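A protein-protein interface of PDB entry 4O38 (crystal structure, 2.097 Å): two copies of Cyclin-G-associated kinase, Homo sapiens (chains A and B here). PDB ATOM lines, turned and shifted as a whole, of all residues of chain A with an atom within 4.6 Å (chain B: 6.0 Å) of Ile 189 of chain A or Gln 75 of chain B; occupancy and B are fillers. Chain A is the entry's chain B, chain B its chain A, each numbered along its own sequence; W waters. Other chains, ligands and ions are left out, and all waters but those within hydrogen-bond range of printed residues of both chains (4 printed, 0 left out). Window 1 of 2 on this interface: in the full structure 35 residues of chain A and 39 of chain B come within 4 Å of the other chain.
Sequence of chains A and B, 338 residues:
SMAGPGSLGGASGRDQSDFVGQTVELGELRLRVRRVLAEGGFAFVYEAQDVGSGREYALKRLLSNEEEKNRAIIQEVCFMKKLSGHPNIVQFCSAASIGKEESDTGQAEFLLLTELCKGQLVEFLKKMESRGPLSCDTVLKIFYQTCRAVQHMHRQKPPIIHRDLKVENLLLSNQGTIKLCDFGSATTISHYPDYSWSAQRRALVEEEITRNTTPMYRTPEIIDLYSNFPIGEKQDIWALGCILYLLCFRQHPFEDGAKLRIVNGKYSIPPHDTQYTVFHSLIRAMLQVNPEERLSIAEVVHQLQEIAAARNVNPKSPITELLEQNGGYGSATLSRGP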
ATOM      1  N   PRO A 158     -16.255  12.268  32.151  1.00  0.00           N
ATOM      2  CA  PRO A 158     -16.358  13.445  31.296  1.00  0.00           C
ATOM      3  C   PRO A 158     -16.426  14.766  32.089  1.00  0.00           C
ATOM      4  O   PRO A 158     -16.692  14.770  33.270  1.00  0.00           O
ATOM      5  CB  PRO A 158     -17.693  13.203  30.548  1.00  0.00           C
ATOM      6  CG  PRO A 158     -18.516  12.466  31.529  1.00  0.00           C
ATOM      7  CD  PRO A 158     -17.576  11.623  32.358  1.00  0.00           C
ATOM      8  N   THR A 188     -23.304  17.156  32.989  1.00  0.00           N
ATOM      9  CA  THR A 188     -22.212  16.401  32.371  1.00  0.00           C
ATOM     10  C   THR A 188     -22.855  15.393  31.387  1.00  0.00           C
ATOM     11  O   THR A 188     -23.997  15.511  31.089  1.00  0.00           O
ATOM     12  CB  THR A 188     -21.334  15.709  33.474  1.00  0.00           C
ATOM     13  OG1 THR A 188     -20.179  15.145  32.886  1.00  0.00           O
ATOM     14  CG2 THR A 188     -22.036  14.628  34.175  1.00  0.00           C
ATOM     15  N   ILE A 189     -22.105  14.408  30.928  1.00  0.00           N
ATOM     16  CA  ILE A 189     -22.639  13.334  30.123  1.00  0.00           C
ATOM     17  C   ILE A 189     -22.677  12.058  30.976  1.00  0.00           C
ATOM     18  O   ILE A 189     -21.666  11.659  31.559  1.00  0.00           O
ATOM     19  CB  ILE A 189     -21.789  13.114  28.911  1.00  0.00           C
ATOM     20  CG1 ILE A 189     -21.919  14.357  28.022  1.00  0.00           C
ATOM     21  CG2 ILE A 189     -22.237  11.855  28.176  1.00  0.00           C
ATOM     22  CD1 ILE A 189     -20.919  14.422  26.929  1.00  0.00           C
ATOM     23  N   SER A 190     -23.846  11.439  31.060  1.00  0.00           N
ATOM     24  CA  SER A 190     -23.964  10.130  31.702  1.00  0.00           C
ATOM     25  C   SER A 190     -23.605   8.994  30.749  1.00  0.00           C
ATOM     26  O   SER A 190     -23.908   9.072  29.558  1.00  0.00           O
ATOM     27  CB  SER A 190     -25.401   9.909  32.142  1.00  0.00           C
ATOM     28  OG  SER A 190     -25.902  11.023  32.890  1.00  0.00           O
ATOM     29  N   HIS A 191     -23.086   7.903  31.327  1.00  0.00           N
ATOM     30  CA  HIS A 191     -22.808   6.630  30.660  1.00  0.00           C
ATOM     31  C   HIS A 191     -21.751   6.865  29.626  1.00  0.00           C
ATOM     32  O   HIS A 191     -21.761   6.285  28.537  1.00  0.00           O
ATOM     33  CB  HIS A 191     -24.080   5.944  30.092  1.00  0.00           C
ATOM     34  CG  HIS A 191     -25.052   5.523  31.155  1.00  0.00           C
ATOM     35  ND1 HIS A 191     -24.764   4.547  32.096  1.00  0.00           N
ATOM     36  CD2 HIS A 191     -26.264   6.025  31.502  1.00  0.00           C
ATOM     37  CE1 HIS A 191     -25.758   4.461  32.959  1.00  0.00           C
ATOM     38  NE2 HIS A 191     -26.682   5.350  32.629  1.00  0.00           N
ATOM     39  N   TYR A 192     -20.801   7.708  30.005  1.00  0.00           N
ATOM     40  CA  TYR A 192     -19.635   7.953  29.202  1.00  0.00           C
ATOM     41  C   TYR A 192     -18.801   6.722  29.413  1.00  0.00           C
ATOM     42  O   TYR A 192     -18.655   6.289  30.560  1.00  0.00           O
ATOM     43  CB  TYR A 192     -18.858   9.138  29.749  1.00  0.00           C
ATOM     44  CG  TYR A 192     -17.951   9.809  28.754  1.00  0.00           C
ATOM     45  CD1 TYR A 192     -18.481  10.493  27.671  1.00  0.00           C
ATOM     46  CD2 TYR A 192     -16.563   9.797  28.911  1.00  0.00           C
ATOM     47  CE1 TYR A 192     -17.667  11.137  26.762  1.00  0.00           C
ATOM     48  CE2 TYR A 192     -15.739  10.438  27.992  1.00  0.00           C
ATOM     49  CZ  TYR A 192     -16.305  11.110  26.922  1.00  0.00           C
ATOM     50  OH  TYR A 192     -15.528  11.755  25.995  1.00  0.00           O
ATOM     51  N   ILE A 231     -18.294  20.746  25.429  1.00  0.00           N
ATOM     52  CA  ILE A 231     -19.652  20.373  25.771  1.00  0.00           C
ATOM     53  C   ILE A 231     -20.245  21.366  26.756  1.00  0.00           C
ATOM     54  O   ILE A 231     -21.172  21.050  27.454  1.00  0.00           O
ATOM     55  CB  ILE A 231     -19.702  18.946  26.381  1.00  0.00           C
ATOM     56  CG1 ILE A 231     -18.786  18.815  27.591  1.00  0.00           C
ATOM     57  CG2 ILE A 231     -19.309  17.921  25.330  1.00  0.00           C
ATOM     58  CD1 ILE A 231     -19.159  17.690  28.535  1.00  0.00           C
ATOM     59  N   ASN B  70     -23.335  19.706  20.899  1.00  0.00           N
ATOM     60  CA  ASN B  70     -22.331  18.643  21.021  1.00  0.00           C
ATOM     61  C   ASN B  70     -22.644  17.758  22.207  1.00  0.00           C
ATOM     62  O   ASN B  70     -22.614  16.507  22.107  1.00  0.00           O
ATOM     63  CB  ASN B  70     -20.915  19.151  21.260  1.00  0.00           C
ATOM     64  CG  ASN B  70     -20.358  19.901  20.088  1.00  0.00           C
ATOM     65  OD1 ASN B  70     -20.891  19.868  18.995  1.00  0.00           O
ATOM     66  ND2 ASN B  70     -19.249  20.606  20.330  1.00  0.00           N
ATOM     67  N   ARG B  71     -22.963  18.395  23.320  1.00  0.00           N
ATOM     68  CA  ARG B  71     -23.236  17.631  24.544  1.00  0.00           C
ATOM     69  C   ARG B  71     -24.460  16.759  24.346  1.00  0.00           C
ATOM     70  O   ARG B  71     -24.470  15.593  24.751  1.00  0.00           O
ATOM     71  CB  ARG B  71     -23.434  18.570  25.766  1.00  0.00           C
ATOM     72  CG  ARG B  71     -23.507  17.813  27.085  1.00  0.00           C
ATOM     73  CD  ARG B  71     -23.632  18.708  28.315  1.00  0.00           C
ATOM     74  NE  ARG B  71     -24.836  19.526  28.292  1.00  0.00           N
ATOM     75  CZ  ARG B  71     -24.907  20.866  28.154  1.00  0.00           C
ATOM     76  NH1 ARG B  71     -26.104  21.436  28.167  1.00  0.00           N
ATOM     77  NH2 ARG B  71     -23.819  21.670  27.987  1.00  0.00           N
ATOM     78  N   ALA B  72     -25.528  17.323  23.782  1.00  0.00           N
ATOM     79  CA  ALA B  72     -26.771  16.545  23.633  1.00  0.00           C
ATOM     80  C   ALA B  72     -26.564  15.344  22.669  1.00  0.00           C
ATOM     81  O   ALA B  72     -27.082  14.264  22.891  1.00  0.00           O
ATOM     82  CB  ALA B  72     -27.928  17.458  23.149  1.00  0.00           C
ATOM     83  N   ILE B  73     -25.779  15.554  21.617  1.00  0.00           N
ATOM     84  CA  ILE B  73     -25.484  14.539  20.685  1.00  0.00           C
ATOM     85  C   ILE B  73     -24.679  13.402  21.300  1.00  0.00           C
ATOM     86  O   ILE B  73     -25.018  12.236  21.147  1.00  0.00           O
ATOM     87  CB  ILE B  73     -24.796  15.096  19.438  1.00  0.00           C
ATOM     88  CG1 ILE B  73     -25.806  15.973  18.638  1.00  0.00           C
ATOM     89  CG2 ILE B  73     -24.336  13.973  18.516  1.00  0.00           C
ATOM     90  CD1 ILE B  73     -25.123  16.893  17.638  1.00  0.00           C
ATOM     91  N   ILE B  74     -23.600  13.740  21.960  1.00  0.00           N
ATOM     92  CA  ILE B  74     -22.755  12.726  22.581  1.00  0.00           C
ATOM     93  C   ILE B  74     -23.558  11.986  23.673  1.00  0.00           C
ATOM     94  O   ILE B  74     -23.412  10.789  23.853  1.00  0.00           O
ATOM     95  CB  ILE B  74     -21.470  13.344  23.159  1.00  0.00           C
ATOM     96  CG1 ILE B  74     -20.613  13.917  22.020  1.00  0.00           C
ATOM     97  CG2 ILE B  74     -20.677  12.313  23.940  1.00  0.00           C
ATOM     98  CD1 ILE B  74     -19.493  14.836  22.468  1.00  0.00           C
ATOM     99  N   GLN B  75     -24.441  12.696  24.351  1.00  0.00           N
ATOM    100  CA  GLN B  75     -25.281  12.065  25.337  1.00  0.00           C
ATOM    101  C   GLN B  75     -26.203  11.015  24.663  1.00  0.00           C
ATOM    102  O   GLN B  75     -26.379   9.929  25.187  1.00  0.00           O
ATOM    103  CB  GLN B  75     -26.082  13.096  26.122  1.00  0.00           C
ATOM    104  CG  GLN B  75     -27.003  12.511  27.172  1.00  0.00           C
ATOM    105  CD  GLN B  75     -26.282  11.794  28.267  1.00  0.00           C
ATOM    106  OE1 GLN B  75     -25.967  12.377  29.317  1.00  0.00           O
ATOM    107  NE2 GLN B  75     -25.960  10.546  28.033  1.00  0.00           N
ATOM    108  N   GLU B  76     -26.756  11.368  23.510  1.00  0.00           N
ATOM    109  CA  GLU B  76     -27.604  10.457  22.794  1.00  0.00           C
ATOM    110  C   GLU B  76     -26.870   9.230  22.402  1.00  0.00           C
ATOM    111  O   GLU B  76     -27.369   8.109  22.588  1.00  0.00           O
ATOM    112  CB  GLU B  76     -28.273  11.127  21.584  1.00  0.00           C
ATOM    113  CG  GLU B  76     -29.069  10.146  20.692  1.00  0.00           C
ATOM    114  CD  GLU B  76     -29.790  10.859  19.540  1.00  0.00           C
ATOM    115  OE1 GLU B  76     -29.870  12.110  19.543  1.00  0.00           O
ATOM    116  OE2 GLU B  76     -30.343  10.165  18.662  1.00  0.00           O
ATOM    117  N   VAL B  77     -25.696   9.409  21.850  1.00  0.00           N
ATOM    118  CA  VAL B  77     -24.831   8.261  21.504  1.00  0.00           C
ATOM    119  C   VAL B  77     -24.557   7.385  22.739  1.00  0.00           C
ATOM    120  O   VAL B  77     -24.608   6.143  22.655  1.00  0.00           O
ATOM    121  CB  VAL B  77     -23.502   8.711  20.889  1.00  0.00           C
ATOM    122  CG1 VAL B  77     -22.551   7.535  20.736  1.00  0.00           C
ATOM    123  CG2 VAL B  77     -23.719   9.449  19.551  1.00  0.00           C
ATOM    124  N   CYS B  78     -24.296   7.990  23.897  1.00  0.00           N
ATOM    125  CA  CYS B  78     -23.945   7.200  25.095  1.00  0.00           C
ATOM    126  C   CYS B  78     -25.192   6.386  25.535  1.00  0.00           C
ATOM    127  O   CYS B  78     -25.066   5.262  25.960  1.00  0.00           O
ATOM    128  CB  CYS B  78     -23.382   8.069  26.262  1.00  0.00           C
ATOM    129  SG  CYS B  78     -21.764   8.787  25.873  1.00  0.00           S
ATOM    130  N   PHE B  79     -26.370   6.949  25.425  1.00  0.00           N
ATOM    131  CA  PHE B  79     -27.565   6.219  25.787  1.00  0.00           C
ATOM    132  C   PHE B  79     -27.807   5.053  24.804  1.00  0.00           C
ATOM    133  O   PHE B  79     -28.157   3.958  25.228  1.00  0.00           O
ATOM    134  CB  PHE B  79     -28.781   7.124  25.876  1.00  0.00           C
ATOM    135  CG  PHE B  79     -28.826   8.004  27.125  1.00  0.00           C
ATOM    136  CD1 PHE B  79     -28.496   7.504  28.366  1.00  0.00           C
ATOM    137  CD2 PHE B  79     -29.277   9.297  27.046  1.00  0.00           C
ATOM    138  CE1 PHE B  79     -28.613   8.286  29.515  1.00  0.00           C
ATOM    139  CE2 PHE B  79     -29.408  10.087  28.200  1.00  0.00           C
ATOM    140  CZ  PHE B  79     -29.061   9.560  29.437  1.00  0.00           C
ATOM    141  N   MET B  80     -27.617   5.305  23.513  1.00  0.00           N
ATOM    142  CA  MET B  80     -27.834   4.252  22.512  1.00  0.00           C
ATOM    143  C   MET B  80     -26.888   3.105  22.823  1.00  0.00           C
ATOM    144  O   MET B  80     -27.294   1.967  22.905  1.00  0.00           O
ATOM    145  CB  MET B  80     -27.687   4.878  21.128  1.00  0.00           C
ATOM    146  CG  MET B  80     -27.623   3.874  20.030  1.00  0.00           C
ATOM    147  SD  MET B  80     -29.423   3.140  19.816  1.00  0.00           S
ATOM    148  CE  MET B  80     -29.379   1.764  21.166  1.00  0.00           C
ATOM    149  N   PHE B 183     -33.301   8.471  21.563  1.00  0.00           N
ATOM    150  CA  PHE B 183     -32.865   8.752  22.913  1.00  0.00           C
ATOM    151  C   PHE B 183     -32.331  10.165  23.053  1.00  0.00           C
ATOM    152  O   PHE B 183     -31.709  10.489  24.071  1.00  0.00           O
ATOM    153  CB  PHE B 183     -31.844   7.694  23.366  1.00  0.00           C
ATOM    154  CG  PHE B 183     -32.375   6.300  23.279  1.00  0.00           C
ATOM    155  CD1 PHE B 183     -33.474   5.935  23.980  1.00  0.00           C
ATOM    156  CD2 PHE B 183     -31.814   5.394  22.387  1.00  0.00           C
ATOM    157  CE1 PHE B 183     -34.013   4.678  23.825  1.00  0.00           C
ATOM    158  CE2 PHE B 183     -32.335   4.149  22.232  1.00  0.00           C
ATOM    159  CZ  PHE B 183     -33.458   3.791  22.932  1.00  0.00           C
ATOM    160  N   ALA B 186     -33.661  11.766  26.258  1.00  0.00           N
ATOM    161  CA  ALA B 186     -33.528  11.000  27.493  1.00  0.00           C
ATOM    162  C   ALA B 186     -32.637  11.693  28.516  1.00  0.00           C
ATOM    163  O   ALA B 186     -31.715  12.418  28.128  1.00  0.00           O
ATOM    164  CB  ALA B 186     -32.933   9.648  27.174  1.00  0.00           C
ATOM    165  N   THR B 188     -30.858  11.019  32.820  1.00  0.00           N
ATOM    166  CA  THR B 188     -30.662  10.181  34.024  1.00  0.00           C
ATOM    167  C   THR B 188     -29.871  11.049  35.051  1.00  0.00           C
ATOM    168  O   THR B 188     -29.745  12.242  34.875  1.00  0.00           O
ATOM    169  CB  THR B 188     -29.913   8.865  33.673  1.00  0.00           C
ATOM    170  OG1 THR B 188     -29.915   7.995  34.807  1.00  0.00           O
ATOM    171  CG2 THR B 188     -28.482   9.096  33.295  1.00  0.00           C
ATOM    172  N   SER B 190     -26.121  11.558  36.681  1.00  0.00           N
ATOM    173  CA  SER B 190     -24.703  11.217  36.663  1.00  0.00           C
ATOM    174  C   SER B 190     -24.099  11.137  38.070  1.00  0.00           C
ATOM    175  O   SER B 190     -24.491  11.905  38.950  1.00  0.00           O
ATOM    176  CB  SER B 190     -23.927  12.290  35.912  1.00  0.00           C
ATOM    177  OG  SER B 190     -24.483  12.561  34.645  1.00  0.00           O
HETATM  178  O   HOH W   1     -26.220  15.345  29.143  1.00  0.00           O
HETATM  179  O   HOH W   2     -22.647   4.496  26.832  1.00  0.00           O
HETATM  180  O   HOH W   3     -25.570  15.098  34.231  1.00  0.00           O
HETATM  181  O   HOH W   4     -28.118  12.468  31.754  1.00  0.00           O
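The side-chain sulfur (SG) of Cys 78 of chain B sits close to the backbone carbonyl oxygen (O) of His 191 of chain A, 3.7 Å away. OE1 of Gln 75 of chain B lies within hydrogen-bond range of N of Ser 190 of chain A (2.9 Å). O of Ile 231 of chain A is in hydrogen-bond range of NH2 of Arg 71 of chain B. OG of Ser 190 of chain A is in hydrogen-bond range of OG of Ser 190 of chain B, at 2.7 Å.
The backbone carbonyl oxygen (O) of Ile 74 of chain B sits at hydrogen-bond distance from the side-chain sulfur (SG) of Cys 78 of chain B.
Among the printed residues, pairs that only touch across the chains: Thr 188 of chain A with Ser 190 of chain B (3.2 Å), Ile 189 of chain A with Arg 71 of chain B (3.9 Å), Ile 189 of chain A with Ile 74 of chain B (3.7 Å), Ile 189 of chain A with Gln 75 of chain B (3.6 Å), Ile 189 of chain A with Cys 78 of chain B (3.9 Å), Ser 190 of chain A with Cys 78 of chain B (3.5 Å), Ser 190 of chain A with Thr 188 of chain B (3.2 Å) and His 191 of chain A with Phe 79 of chain B (3.8 Å).
Of the printed residues of chain B, Ile 189 of chain A touches Arg 71 (3.9 Å), Ile 74 (3.7 Å), Gln 75 (3.6 Å) and Cys 78 (3.9 Å). Gln 75 of chain B touches just these residues of chain A: Ile 189 and Ser 190. Printed residues of chain A within 4 Å of Arg 71 of chain B: Ile 189 and Ile 231. Printed residues of chain B within 4 Å of His 191 of chain A: Cys 78 (3.3 Å) and Phe 79 (3.8 Å). Printed residues of chain A within 4 Å of Ser 190 of chain B: Thr 188 and Ser 190. Printed residues of chain B within 4 Å of Ser 190 of chain A: Gln 75 (2.9 Å), Cys 78 (3.5 Å), Thr 188 (3.2 Å) and Ser 190 (2.7 Å). Printed residues of chain A within 4 Å of Thr 188 of chain B: Ser 190. Met 80 of chain B touches none of the printed residues of chain A. Tyr 192 of chain A touches none of the printed residues of chain B. The nearest residue of chain B that does not touch Ile 189 of chain A is Ser 190 of chain B (4.1 Å). The nearest printed residue of chain B that does not touch Ser 190 of chain A is Phe 79 of chain B (4.5 Å).
Printed residues of chain A that touch a printed residue of chain B: Thr 188, Ile 189, Ser 190, His 191 and Ile 231. Hydrophobic or aromatic side chains of chain B within 4 Å of the printed part of chain A: Ile 74 and Phe 79. Among the printed residues, no Asp or Glu carboxylate lies within 4 Å of a Lys or Arg side-chain nitrogen of the other chain.
Thr 188 of chain A touches Ser 190 of chain B, and with the chains exchanged Ser 190 of chain A touches Thr 188 of chain B. Ser 190 of chain B touches its own counterpart, Ser 190 of chain A. Of the 12 pairs that touch across the chains among the printed residues, 3 have their exchanged pair printed and touching as well.
Water W2 lies within hydrogen-bond range of the backbone carbonyl oxygen of His 191 of chain A (2.6 Å) and the backbone carbonyl oxygen of Cys 78 of chain B (2.7 Å). Water W3 bridges OG of Ser 190 of chain B (2.8 Å) and N of Thr 188 of chain A (3.3 Å). Water W4 lies within hydrogen-bond range of OG of Ser 190 of chain A (2.9 Å), OE1 of Gln 75 of chain B (3.3 Å) and N of Thr 188 of chain B (3.3 Å). Water W1 bridges O of Thr 188 of chain A (3.0 Å) and OE1 of Gln 75 of chain B (3.0 Å).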
